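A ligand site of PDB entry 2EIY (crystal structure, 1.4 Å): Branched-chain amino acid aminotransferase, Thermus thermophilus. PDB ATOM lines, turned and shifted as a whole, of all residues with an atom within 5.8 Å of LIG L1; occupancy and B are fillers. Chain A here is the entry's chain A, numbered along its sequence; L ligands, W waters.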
ATOM      1  N   PHE A  36      27.771  15.759  12.893  1.00  0.00           N
ATOM      2  CA  PHE A  36      28.403  16.533  13.953  1.00  0.00           C
ATOM      3  C   PHE A  36      27.444  16.837  15.074  1.00  0.00           C
ATOM      4  O   PHE A  36      26.255  16.518  15.003  1.00  0.00           O
ATOM      5  CB  PHE A  36      28.966  17.849  13.379  1.00  0.00           C
ATOM      6  CG  PHE A  36      27.905  18.809  12.889  1.00  0.00           C
ATOM      7  CD1 PHE A  36      27.294  19.709  13.759  1.00  0.00           C
ATOM      8  CD2 PHE A  36      27.526  18.813  11.551  1.00  0.00           C
ATOM      9  CE1 PHE A  36      26.320  20.589  13.306  1.00  0.00           C
ATOM     10  CE2 PHE A  36      26.550  19.691  11.085  1.00  0.00           C
ATOM     11  CZ  PHE A  36      25.944  20.586  11.962  1.00  0.00           C
ATOM     12  N   GLU A  37      27.980  17.443  16.124  1.00  0.00           N
ATOM     13  CA  GLU A  37      27.174  17.857  17.259  1.00  0.00           C
ATOM     14  C   GLU A  37      27.636  19.220  17.719  1.00  0.00           C
ATOM     15  O   GLU A  37      28.703  19.705  17.330  1.00  0.00           O
ATOM     16  CB  GLU A  37      27.277  16.853  18.419  1.00  0.00           C
ATOM     17  CG  GLU A  37      26.197  15.776  18.364  1.00  0.00           C
ATOM     18  CD  GLU A  37      24.790  16.352  18.454  1.00  0.00           C
ATOM     19  OE1 GLU A  37      23.851  15.734  17.923  1.00  0.00           O
ATOM     20  OE2 GLU A  37      24.625  17.423  19.082  1.00  0.00           O
ATOM     21  N   GLY A  38      26.784  19.854  18.513  1.00  0.00           N
ATOM     22  CA  GLY A  38      27.083  21.151  19.072  1.00  0.00           C
ATOM     23  C   GLY A  38      26.835  20.970  20.550  1.00  0.00           C
ATOM     24  O   GLY A  38      25.702  20.741  20.965  1.00  0.00           O
ATOM     25  N   HIS A  56      23.587  14.417  23.750  1.00  0.00           N
ATOM     26  CA  HIS A  56      24.272  14.865  22.547  1.00  0.00           C
ATOM     27  C   HIS A  56      25.055  13.726  21.906  1.00  0.00           C
ATOM     28  O   HIS A  56      25.061  13.582  20.675  1.00  0.00           O
ATOM     29  CB  HIS A  56      25.202  16.041  22.859  1.00  0.00           C
ATOM     30  CG  HIS A  56      24.502  17.360  22.905  1.00  0.00           C
ATOM     31  ND1 HIS A  56      24.077  18.007  21.764  1.00  0.00           N
ATOM     32  CD2 HIS A  56      24.132  18.147  23.944  1.00  0.00           C
ATOM     33  CE1 HIS A  56      23.468  19.131  22.097  1.00  0.00           C
ATOM     34  NE2 HIS A  56      23.479  19.237  23.416  1.00  0.00           N
ATOM     35  N   ARG A  59      22.706  11.360  20.143  1.00  0.00           N
ATOM     36  CA  ARG A  59      22.254  11.875  18.862  1.00  0.00           C
ATOM     37  C   ARG A  59      23.364  11.786  17.808  1.00  0.00           C
ATOM     38  O   ARG A  59      23.095  11.570  16.629  1.00  0.00           O
ATOM     39  CB  ARG A  59      21.773  13.319  19.003  1.00  0.00           C
ATOM     40  CG  ARG A  59      21.044  13.825  17.767  1.00  0.00           C
ATOM     41  CD  ARG A  59      20.298  15.132  18.045  1.00  0.00           C
ATOM     42  NE  ARG A  59      21.202  16.221  18.393  1.00  0.00           N
ATOM     43  CZ  ARG A  59      20.802  17.385  18.876  1.00  0.00           C
ATOM     44  NH1 ARG A  59      19.506  17.620  19.086  1.00  0.00           N
ATOM     45  NH2 ARG A  59      21.695  18.337  19.140  1.00  0.00           N
ATOM     46  N   ARG A 148      12.678  24.110   4.293  1.00  0.00           N
ATOM     47  CA  ARG A 148      13.379  23.050   5.011  1.00  0.00           C
ATOM     48  C   ARG A 148      13.000  21.776   4.254  1.00  0.00           C
ATOM     49  O   ARG A 148      11.846  21.584   3.876  1.00  0.00           O
ATOM     50  CB  ARG A 148      12.883  22.988   6.459  1.00  0.00           C
ATOM     51  CG  ARG A 148      13.351  21.775   7.266  1.00  0.00           C
ATOM     52  CD  ARG A 148      14.707  21.972   7.885  1.00  0.00           C
ATOM     53  NE  ARG A 148      15.087  20.866   8.775  1.00  0.00           N
ATOM     54  CZ  ARG A 148      16.292  20.733   9.310  1.00  0.00           C
ATOM     55  NH1 ARG A 148      17.227  21.633   9.054  1.00  0.00           N
ATOM     56  NH2 ARG A 148      16.576  19.692  10.085  1.00  0.00           N
ATOM     57  N   LYS A 159      22.071  15.522  12.389  1.00  0.00           N
ATOM     58  CA  LYS A 159      22.953  16.634  12.061  1.00  0.00           C
ATOM     59  C   LYS A 159      23.947  16.116  11.037  1.00  0.00           C
ATOM     60  O   LYS A 159      25.109  15.850  11.356  1.00  0.00           O
ATOM     61  CB  LYS A 159      23.683  17.158  13.305  1.00  0.00           C
ATOM     62  CG  LYS A 159      22.827  18.003  14.249  1.00  0.00           C
ATOM     63  CD  LYS A 159      23.739  18.760  15.216  1.00  0.00           C
ATOM     64  CE  LYS A 159      22.970  19.615  16.210  1.00  0.00           C
ATOM     65  NZ  LYS A 159      22.013  20.508  15.544  1.00  0.00           N
ATOM     66  N   TYR A 164      23.201  21.089   5.927  1.00  0.00           N
ATOM     67  CA  TYR A 164      23.440  22.493   6.166  1.00  0.00           C
ATOM     68  C   TYR A 164      23.658  23.417   4.993  1.00  0.00           C
ATOM     69  O   TYR A 164      23.868  24.617   5.166  1.00  0.00           O
ATOM     70  CB  TYR A 164      24.512  22.638   7.269  1.00  0.00           C
ATOM     71  CG  TYR A 164      23.964  22.008   8.528  1.00  0.00           C
ATOM     72  CD1 TYR A 164      23.944  20.614   8.677  1.00  0.00           C
ATOM     73  CD2 TYR A 164      23.261  22.769   9.478  1.00  0.00           C
ATOM     74  CE1 TYR A 164      23.243  19.999   9.706  1.00  0.00           C
ATOM     75  CE2 TYR A 164      22.545  22.162  10.509  1.00  0.00           C
ATOM     76  CZ  TYR A 164      22.536  20.772  10.613  1.00  0.00           C
ATOM     77  OH  TYR A 164      21.780  20.142  11.567  1.00  0.00           O
ATOM     78  N   SER A 167      20.558  25.238   5.302  1.00  0.00           N
ATOM     79  CA  SER A 167      20.656  26.223   6.373  1.00  0.00           C
ATOM     80  C   SER A 167      21.529  27.416   5.944  1.00  0.00           C
ATOM     81  O   SER A 167      21.193  28.572   6.224  1.00  0.00           O
ATOM     82  CB  SER A 167      21.255  25.604   7.635  1.00  0.00           C
ATOM     83  OG  SER A 167      20.369  24.657   8.205  1.00  0.00           O
ATOM     84  N   GLU A 193      11.455  25.769  11.106  1.00  0.00           N
ATOM     85  CA  GLU A 193      12.373  26.232  12.154  1.00  0.00           C
ATOM     86  C   GLU A 193      13.366  27.239  11.589  1.00  0.00           C
ATOM     87  O   GLU A 193      13.290  27.602  10.416  1.00  0.00           O
ATOM     88  CB  GLU A 193      13.132  25.049  12.768  1.00  0.00           C
ATOM     89  CG  GLU A 193      14.013  24.274  11.805  1.00  0.00           C
ATOM     90  CD  GLU A 193      15.096  23.518  12.536  1.00  0.00           C
ATOM     91  OE1 GLU A 193      15.956  24.182  13.140  1.00  0.00           O
ATOM     92  OE2 GLU A 193      15.098  22.270  12.515  1.00  0.00           O
ATOM     93  N   GLY A 194      14.272  27.708  12.437  1.00  0.00           N
ATOM     94  CA  GLY A 194      15.279  28.651  11.985  1.00  0.00           C
ATOM     95  C   GLY A 194      16.378  27.883  11.282  1.00  0.00           C
ATOM     96  O   GLY A 194      16.320  26.657  11.203  1.00  0.00           O
ATOM     97  N   SER A 195      17.392  28.578  10.763  1.00  0.00           N
ATOM     98  CA  SER A 195      18.467  27.877  10.070  1.00  0.00           C
ATOM     99  C   SER A 195      19.195  26.926  11.024  1.00  0.00           C
ATOM    100  O   SER A 195      19.817  25.953  10.600  1.00  0.00           O
ATOM    101  CB  SER A 195      19.459  28.866   9.450  1.00  0.00           C
ATOM    102  OG  SER A 195      20.269  29.478  10.442  1.00  0.00           O
ATOM    103  N   GLY A 196      19.100  27.216  12.325  1.00  0.00           N
ATOM    104  CA  GLY A 196      19.750  26.377  13.315  1.00  0.00           C
ATOM    105  C   GLY A 196      19.128  26.494  14.698  1.00  0.00           C
ATOM    106  O   GLY A 196      19.823  26.362  15.718  1.00  0.00           O
ATOM    107  N   GLU A 197      17.824  26.737  14.736  1.00  0.00           N
ATOM    108  CA  GLU A 197      17.109  26.889  15.993  1.00  0.00           C
ATOM    109  C   GLU A 197      15.671  26.398  15.895  1.00  0.00           C
ATOM    110  O   GLU A 197      15.046  26.520  14.850  1.00  0.00           O
ATOM    111  CB  GLU A 197      17.050  28.373  16.401  1.00  0.00           C
ATOM    112  CG  GLU A 197      18.360  29.123  16.411  1.00  0.00           C
ATOM    113  CD  GLU A 197      18.659  29.847  15.103  1.00  0.00           C
ATOM    114  OE1 GLU A 197      19.548  30.727  15.116  1.00  0.00           O
ATOM    115  OE2 GLU A 197      18.033  29.532  14.063  1.00  0.00           O
ATOM    116  N   ASN A 198      15.161  25.842  16.988  1.00  0.00           N
ATOM    117  CA  ASN A 198      13.770  25.405  17.028  1.00  0.00           C
ATOM    118  C   ASN A 198      12.937  26.625  17.437  1.00  0.00           C
ATOM    119  O   ASN A 198      13.452  27.534  18.098  1.00  0.00           O
ATOM    120  CB  ASN A 198      13.584  24.275  18.039  1.00  0.00           C
ATOM    121  CG  ASN A 198      14.228  22.982  17.596  1.00  0.00           C
ATOM    122  OD1 ASN A 198      14.875  22.298  18.382  1.00  0.00           O
ATOM    123  ND2 ASN A 198      14.041  22.624  16.326  1.00  0.00           N
ATOM    124  N   LEU A 216      14.890  19.418  13.525  1.00  0.00           N
ATOM    125  CA  LEU A 216      15.733  18.595  14.374  1.00  0.00           C
ATOM    126  C   LEU A 216      15.064  18.605  15.747  1.00  0.00           C
ATOM    127  O   LEU A 216      14.488  19.628  16.137  1.00  0.00           O
ATOM    128  CB  LEU A 216      17.136  19.180  14.496  1.00  0.00           C
ATOM    129  CG  LEU A 216      18.098  18.185  15.136  1.00  0.00           C
ATOM    130  CD1 LEU A 216      18.771  17.380  14.044  1.00  0.00           C
ATOM    131  CD2 LEU A 216      19.130  18.901  15.966  1.00  0.00           C
ATOM    132  N   GLU A 217      15.109  17.486  16.461  1.00  0.00           N
ATOM    133  CA  GLU A 217      14.517  17.408  17.803  1.00  0.00           C
ATOM    134  C   GLU A 217      15.532  18.037  18.760  1.00  0.00           C
ATOM    135  O   GLU A 217      16.393  17.356  19.310  1.00  0.00           O
ATOM    136  CB  GLU A 217      14.271  15.957  18.211  1.00  0.00           C
ATOM    137  CG  GLU A 217      13.286  15.201  17.335  1.00  0.00           C
ATOM    138  CD  GLU A 217      13.121  13.764  17.772  1.00  0.00           C
ATOM    139  OE1 GLU A 217      12.186  13.092  17.282  1.00  0.00           O
ATOM    140  OE2 GLU A 217      13.928  13.292  18.602  1.00  0.00           O
ATOM    141  N   GLY A 218      15.418  19.348  18.958  1.00  0.00           N
ATOM    142  CA  GLY A 218      16.364  20.041  19.812  1.00  0.00           C
ATOM    143  C   GLY A 218      16.414  19.653  21.280  1.00  0.00           C
ATOM    144  O   GLY A 218      15.392  19.418  21.915  1.00  0.00           O
ATOM    145  N   ILE A 219      17.632  19.601  21.811  1.00  0.00           N
ATOM    146  CA  ILE A 219      17.837  19.282  23.203  1.00  0.00           C
ATOM    147  C   ILE A 219      17.528  20.545  24.029  1.00  0.00           C
ATOM    148  O   ILE A 219      17.052  20.463  25.151  1.00  0.00           O
ATOM    149  CB  ILE A 219      19.292  18.789  23.429  1.00  0.00           C
ATOM    150  CG1 ILE A 219      19.414  17.386  22.829  1.00  0.00           C
ATOM    151  CG2 ILE A 219      19.634  18.784  24.916  1.00  0.00           C
ATOM    152  CD1 ILE A 219      20.836  16.891  22.692  1.00  0.00           C
ATOM    153  N   THR A 220      17.770  21.722  23.443  1.00  0.00           N
ATOM    154  CA  THR A 220      17.464  22.968  24.140  1.00  0.00           C
ATOM    155  C   THR A 220      15.937  23.094  24.190  1.00  0.00           C
ATOM    156  O   THR A 220      15.371  23.470  25.211  1.00  0.00           O
ATOM    157  CB  THR A 220      18.077  24.180  23.426  1.00  0.00           C
ATOM    158  OG1 THR A 220      19.448  23.896  23.115  1.00  0.00           O
ATOM    159  CG2 THR A 220      18.033  25.414  24.327  1.00  0.00           C
ATOM    160  N   ARG A 221      15.282  22.744  23.087  1.00  0.00           N
ATOM    161  CA  ARG A 221      13.820  22.767  23.015  1.00  0.00           C
ATOM    162  C   ARG A 221      13.261  21.860  24.112  1.00  0.00           C
ATOM    163  O   ARG A 221      12.336  22.224  24.846  1.00  0.00           O
ATOM    164  CB  ARG A 221      13.364  22.264  21.638  1.00  0.00           C
ATOM    165  CG  ARG A 221      11.862  21.996  21.497  1.00  0.00           C
ATOM    166  CD  ARG A 221      11.563  21.386  20.135  1.00  0.00           C
ATOM    167  NE  ARG A 221      10.128  21.194  19.910  1.00  0.00           N
ATOM    168  CZ  ARG A 221       9.400  20.230  20.464  1.00  0.00           C
ATOM    169  NH1 ARG A 221       9.957  19.343  21.279  1.00  0.00           N
ATOM    170  NH2 ARG A 221       8.104  20.147  20.190  1.00  0.00           N
ATOM    171  N   THR A 254      15.258  28.355  20.218  1.00  0.00           N
ATOM    172  CA  THR A 254      16.145  27.614  21.102  1.00  0.00           C
ATOM    173  C   THR A 254      17.173  26.811  20.306  1.00  0.00           C
ATOM    174  O   THR A 254      16.921  26.380  19.190  1.00  0.00           O
ATOM    175  CB  THR A 254      15.378  26.635  22.024  1.00  0.00           C
ATOM    176  OG1 THR A 254      14.732  25.633  21.221  1.00  0.00           O
ATOM    177  CG2 THR A 254      14.330  27.378  22.844  1.00  0.00           C
ATOM    178  N   GLY A 255      18.349  26.632  20.908  1.00  0.00           N
ATOM    179  CA  GLY A 255      19.415  25.886  20.272  1.00  0.00           C
ATOM    180  C   GLY A 255      20.605  25.915  21.196  1.00  0.00           C
ATOM    181  O   GLY A 255      20.698  26.788  22.072  1.00  0.00           O
ATOM    182  N   THR A 256      21.533  24.981  21.042  1.00  0.00           N
ATOM    183  CA  THR A 256      22.705  24.958  21.909  1.00  0.00           C
ATOM    184  C   THR A 256      23.473  26.278  21.800  1.00  0.00           C
ATOM    185  O   THR A 256      23.817  26.881  22.816  1.00  0.00           O
ATOM    186  CB  THR A 256      23.609  23.764  21.572  1.00  0.00           C
ATOM    187  OG1 THR A 256      22.908  22.551  21.890  1.00  0.00           O
ATOM    188  CG2 THR A 256      24.898  23.821  22.383  1.00  0.00           C
ATOM    189  N   ALA A 257      23.726  26.719  20.573  1.00  0.00           N
ATOM    190  CA  ALA A 257      24.448  27.978  20.362  1.00  0.00           C
ATOM    191  C   ALA A 257      23.563  29.191  20.672  1.00  0.00           C
ATOM    192  O   ALA A 257      24.032  30.195  21.207  1.00  0.00           O
ATOM    193  CB  ALA A 257      24.953  28.054  18.933  1.00  0.00           C
HETATM  194  N1  LIG L   1      17.924  23.096  14.306  1.00  0.00           N
HETATM  195  C1  LIG L   1      18.914  22.549  13.560  1.00  0.00           C
HETATM  196  C2  LIG L   1      18.715  22.471  12.045  1.00  0.00           C
HETATM  197  C3  LIG L   1      20.048  22.095  14.178  1.00  0.00           C
HETATM  198  O1  LIG L   1      21.067  21.539  13.436  1.00  0.00           O
HETATM  199  C4  LIG L   1      20.189  22.178  15.551  1.00  0.00           C
HETATM  200  C5  LIG L   1      21.473  21.605  16.180  1.00  0.00           C
HETATM  201  C6  LIG L   1      19.142  22.749  16.311  1.00  0.00           C
HETATM  202  C7  LIG L   1      18.027  23.198  15.662  1.00  0.00           C
HETATM  203  C8  LIG L   1      19.167  22.933  17.835  1.00  0.00           C
HETATM  204  O2  LIG L   1      19.204  21.720  18.539  1.00  0.00           O
HETATM  205  P1  LIG L   1      19.861  21.704  19.999  1.00  0.00           P
HETATM  206  O3  LIG L   1      21.249  22.237  19.920  1.00  0.00           O
HETATM  207  O4  LIG L   1      19.875  20.179  20.337  1.00  0.00           O
HETATM  208  O5  LIG L   1      18.918  22.418  20.899  1.00  0.00           O
HETATM  209  C1  LG2 L   2      24.462  23.827  16.416  1.00  0.00           C
HETATM  210  C2  LG2 L   2      24.228  24.791  15.252  1.00  0.00           C
HETATM  211  C3  LG2 L   2      24.057  24.116  13.884  1.00  0.00           C
HETATM  212  C4  LG2 L   2      22.898  24.773  13.140  1.00  0.00           C
HETATM  213  C5  LG2 L   2      25.342  24.268  13.072  1.00  0.00           C
HETATM  214  C6  LG2 L   2      24.403  24.479  17.787  1.00  0.00           C
HETATM  215  O1  LG2 L   2      25.432  24.429  18.471  1.00  0.00           O
HETATM  216  O2  LG2 L   2      23.339  25.018  18.178  1.00  0.00           O
HETATM  217  O   HOH W   1      16.435  23.385  20.426  1.00  0.00           O
HETATM  218  O   HOH W   2      23.535  20.762  19.170  1.00  0.00           O
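Arg 148 touches LIG L1. O of Ser 195 touches C2 of LIG L1 (3.9 Å). Gly 196 touches LIG L1. Glu 197 touches LIG L1 (N to C7, 3.7 Å). Leu 216 touches LIG L1. Gly 218 touches LIG L1. CA of Gly 255 touches O5 of LIG L1, 3.6 Å away. Hydrophobic or aromatic side chains within 4 Å of LIG L1: Tyr 164, Leu 216 and Ile 219. 14 residues have an atom within 4 Å of LIG L1: Arg 59, Arg 148, Lys 159, Tyr 164, Glu 193, Ser 195, Gly 196, Glu 197, Leu 216, Gly 218, Ile 219, Thr 220, Gly 255 and Thr 256. Along chain A the residues within 4 Å of LIG L1 span positions 59 to 256.
Water W1 lies within hydrogen-bond range of O5 of LIG L1 (2.7 Å), OD1 of Asn 198 (2.8 Å), OG1 of Thr 254 (2.9 Å) and N of Arg 221 (3.0 Å). Water W2 lies within hydrogen-bond range of the backbone carbonyl oxygen (O) of Gly 38 (2.8 Å), an oxygen (O3) of LIG L1 (2.8 Å), the guanidinium group (NH2) of Arg 59 (3.0 Å) and the side-chain hydroxyl (OG1) of Thr 256 (3.3 Å).
The backbone NH (N) of Phe 36 lies within hydrogen-bond range of the backbone carbonyl oxygen (O) of Lys 159 (3.1 Å). OE2 of Glu 193 is in salt-bridge range of NH2 of Arg 148 (3.8 Å). The backbone NH of Leu 216 is in hydrogen-bond range of the side-chain carboxylate of Glu 193. N of Thr 256 is in hydrogen-bond range of OG1 of Thr 220. The side-chain hydroxyl (OG1) of Thr 220 sits close to the backbone carbonyl oxygen (O) of Gly 255 (3.3 Å). NE of Arg 59 lies within salt-bridge range of OE1 of Glu 37, at 2.7 Å. OD1 of Asn 198 lies within hydrogen-bond range of N of Gly 218. N of Ser 195 lies within hydrogen-bond range of OE2 of Glu 197.
A carbon (C5) of LIG L1 is covalently linked to the side-chain amino group of Lys 159, 1.4 Å away. OH of Tyr 164 sits at hydrogen-bond distance from O1 of LIG L1 (2.4 Å). The side-chain carboxylate (OE1) of Glu 193 sits at hydrogen-bond distance from a nitrogen (N1) of LIG L1. O3 of LIG L1 sits at hydrogen-bond distance from N of Thr 256. The side-chain hydroxyl (OG1) of Thr 256 lies within hydrogen-bond range of an oxygen (O3) of LIG L1, 2.6 Å away. An oxygen (O5) of LIG L1 is in hydrogen-bond range of the backbone NH (N) of Thr 220 (2.9 Å). The side-chain hydroxyl of Thr 220 lies within hydrogen-bond range of an oxygen (O5) of LIG L1, 2.7 Å away. The backbone NH (N) of Ile 219 is in hydrogen-bond range of an oxygen (O4) of LIG L1 (2.7 Å). NH2 of Arg 59 lies within salt-bridge range of O4 of LIG L1. N of Thr 256 lies within hydrogen-bond range of O2 of LG2 L2, 3.4 Å away. The backbone NH (N) of Ala 257 is in hydrogen-bond range of an oxygen (O2) of LG2 L2, at 3.0 Å.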
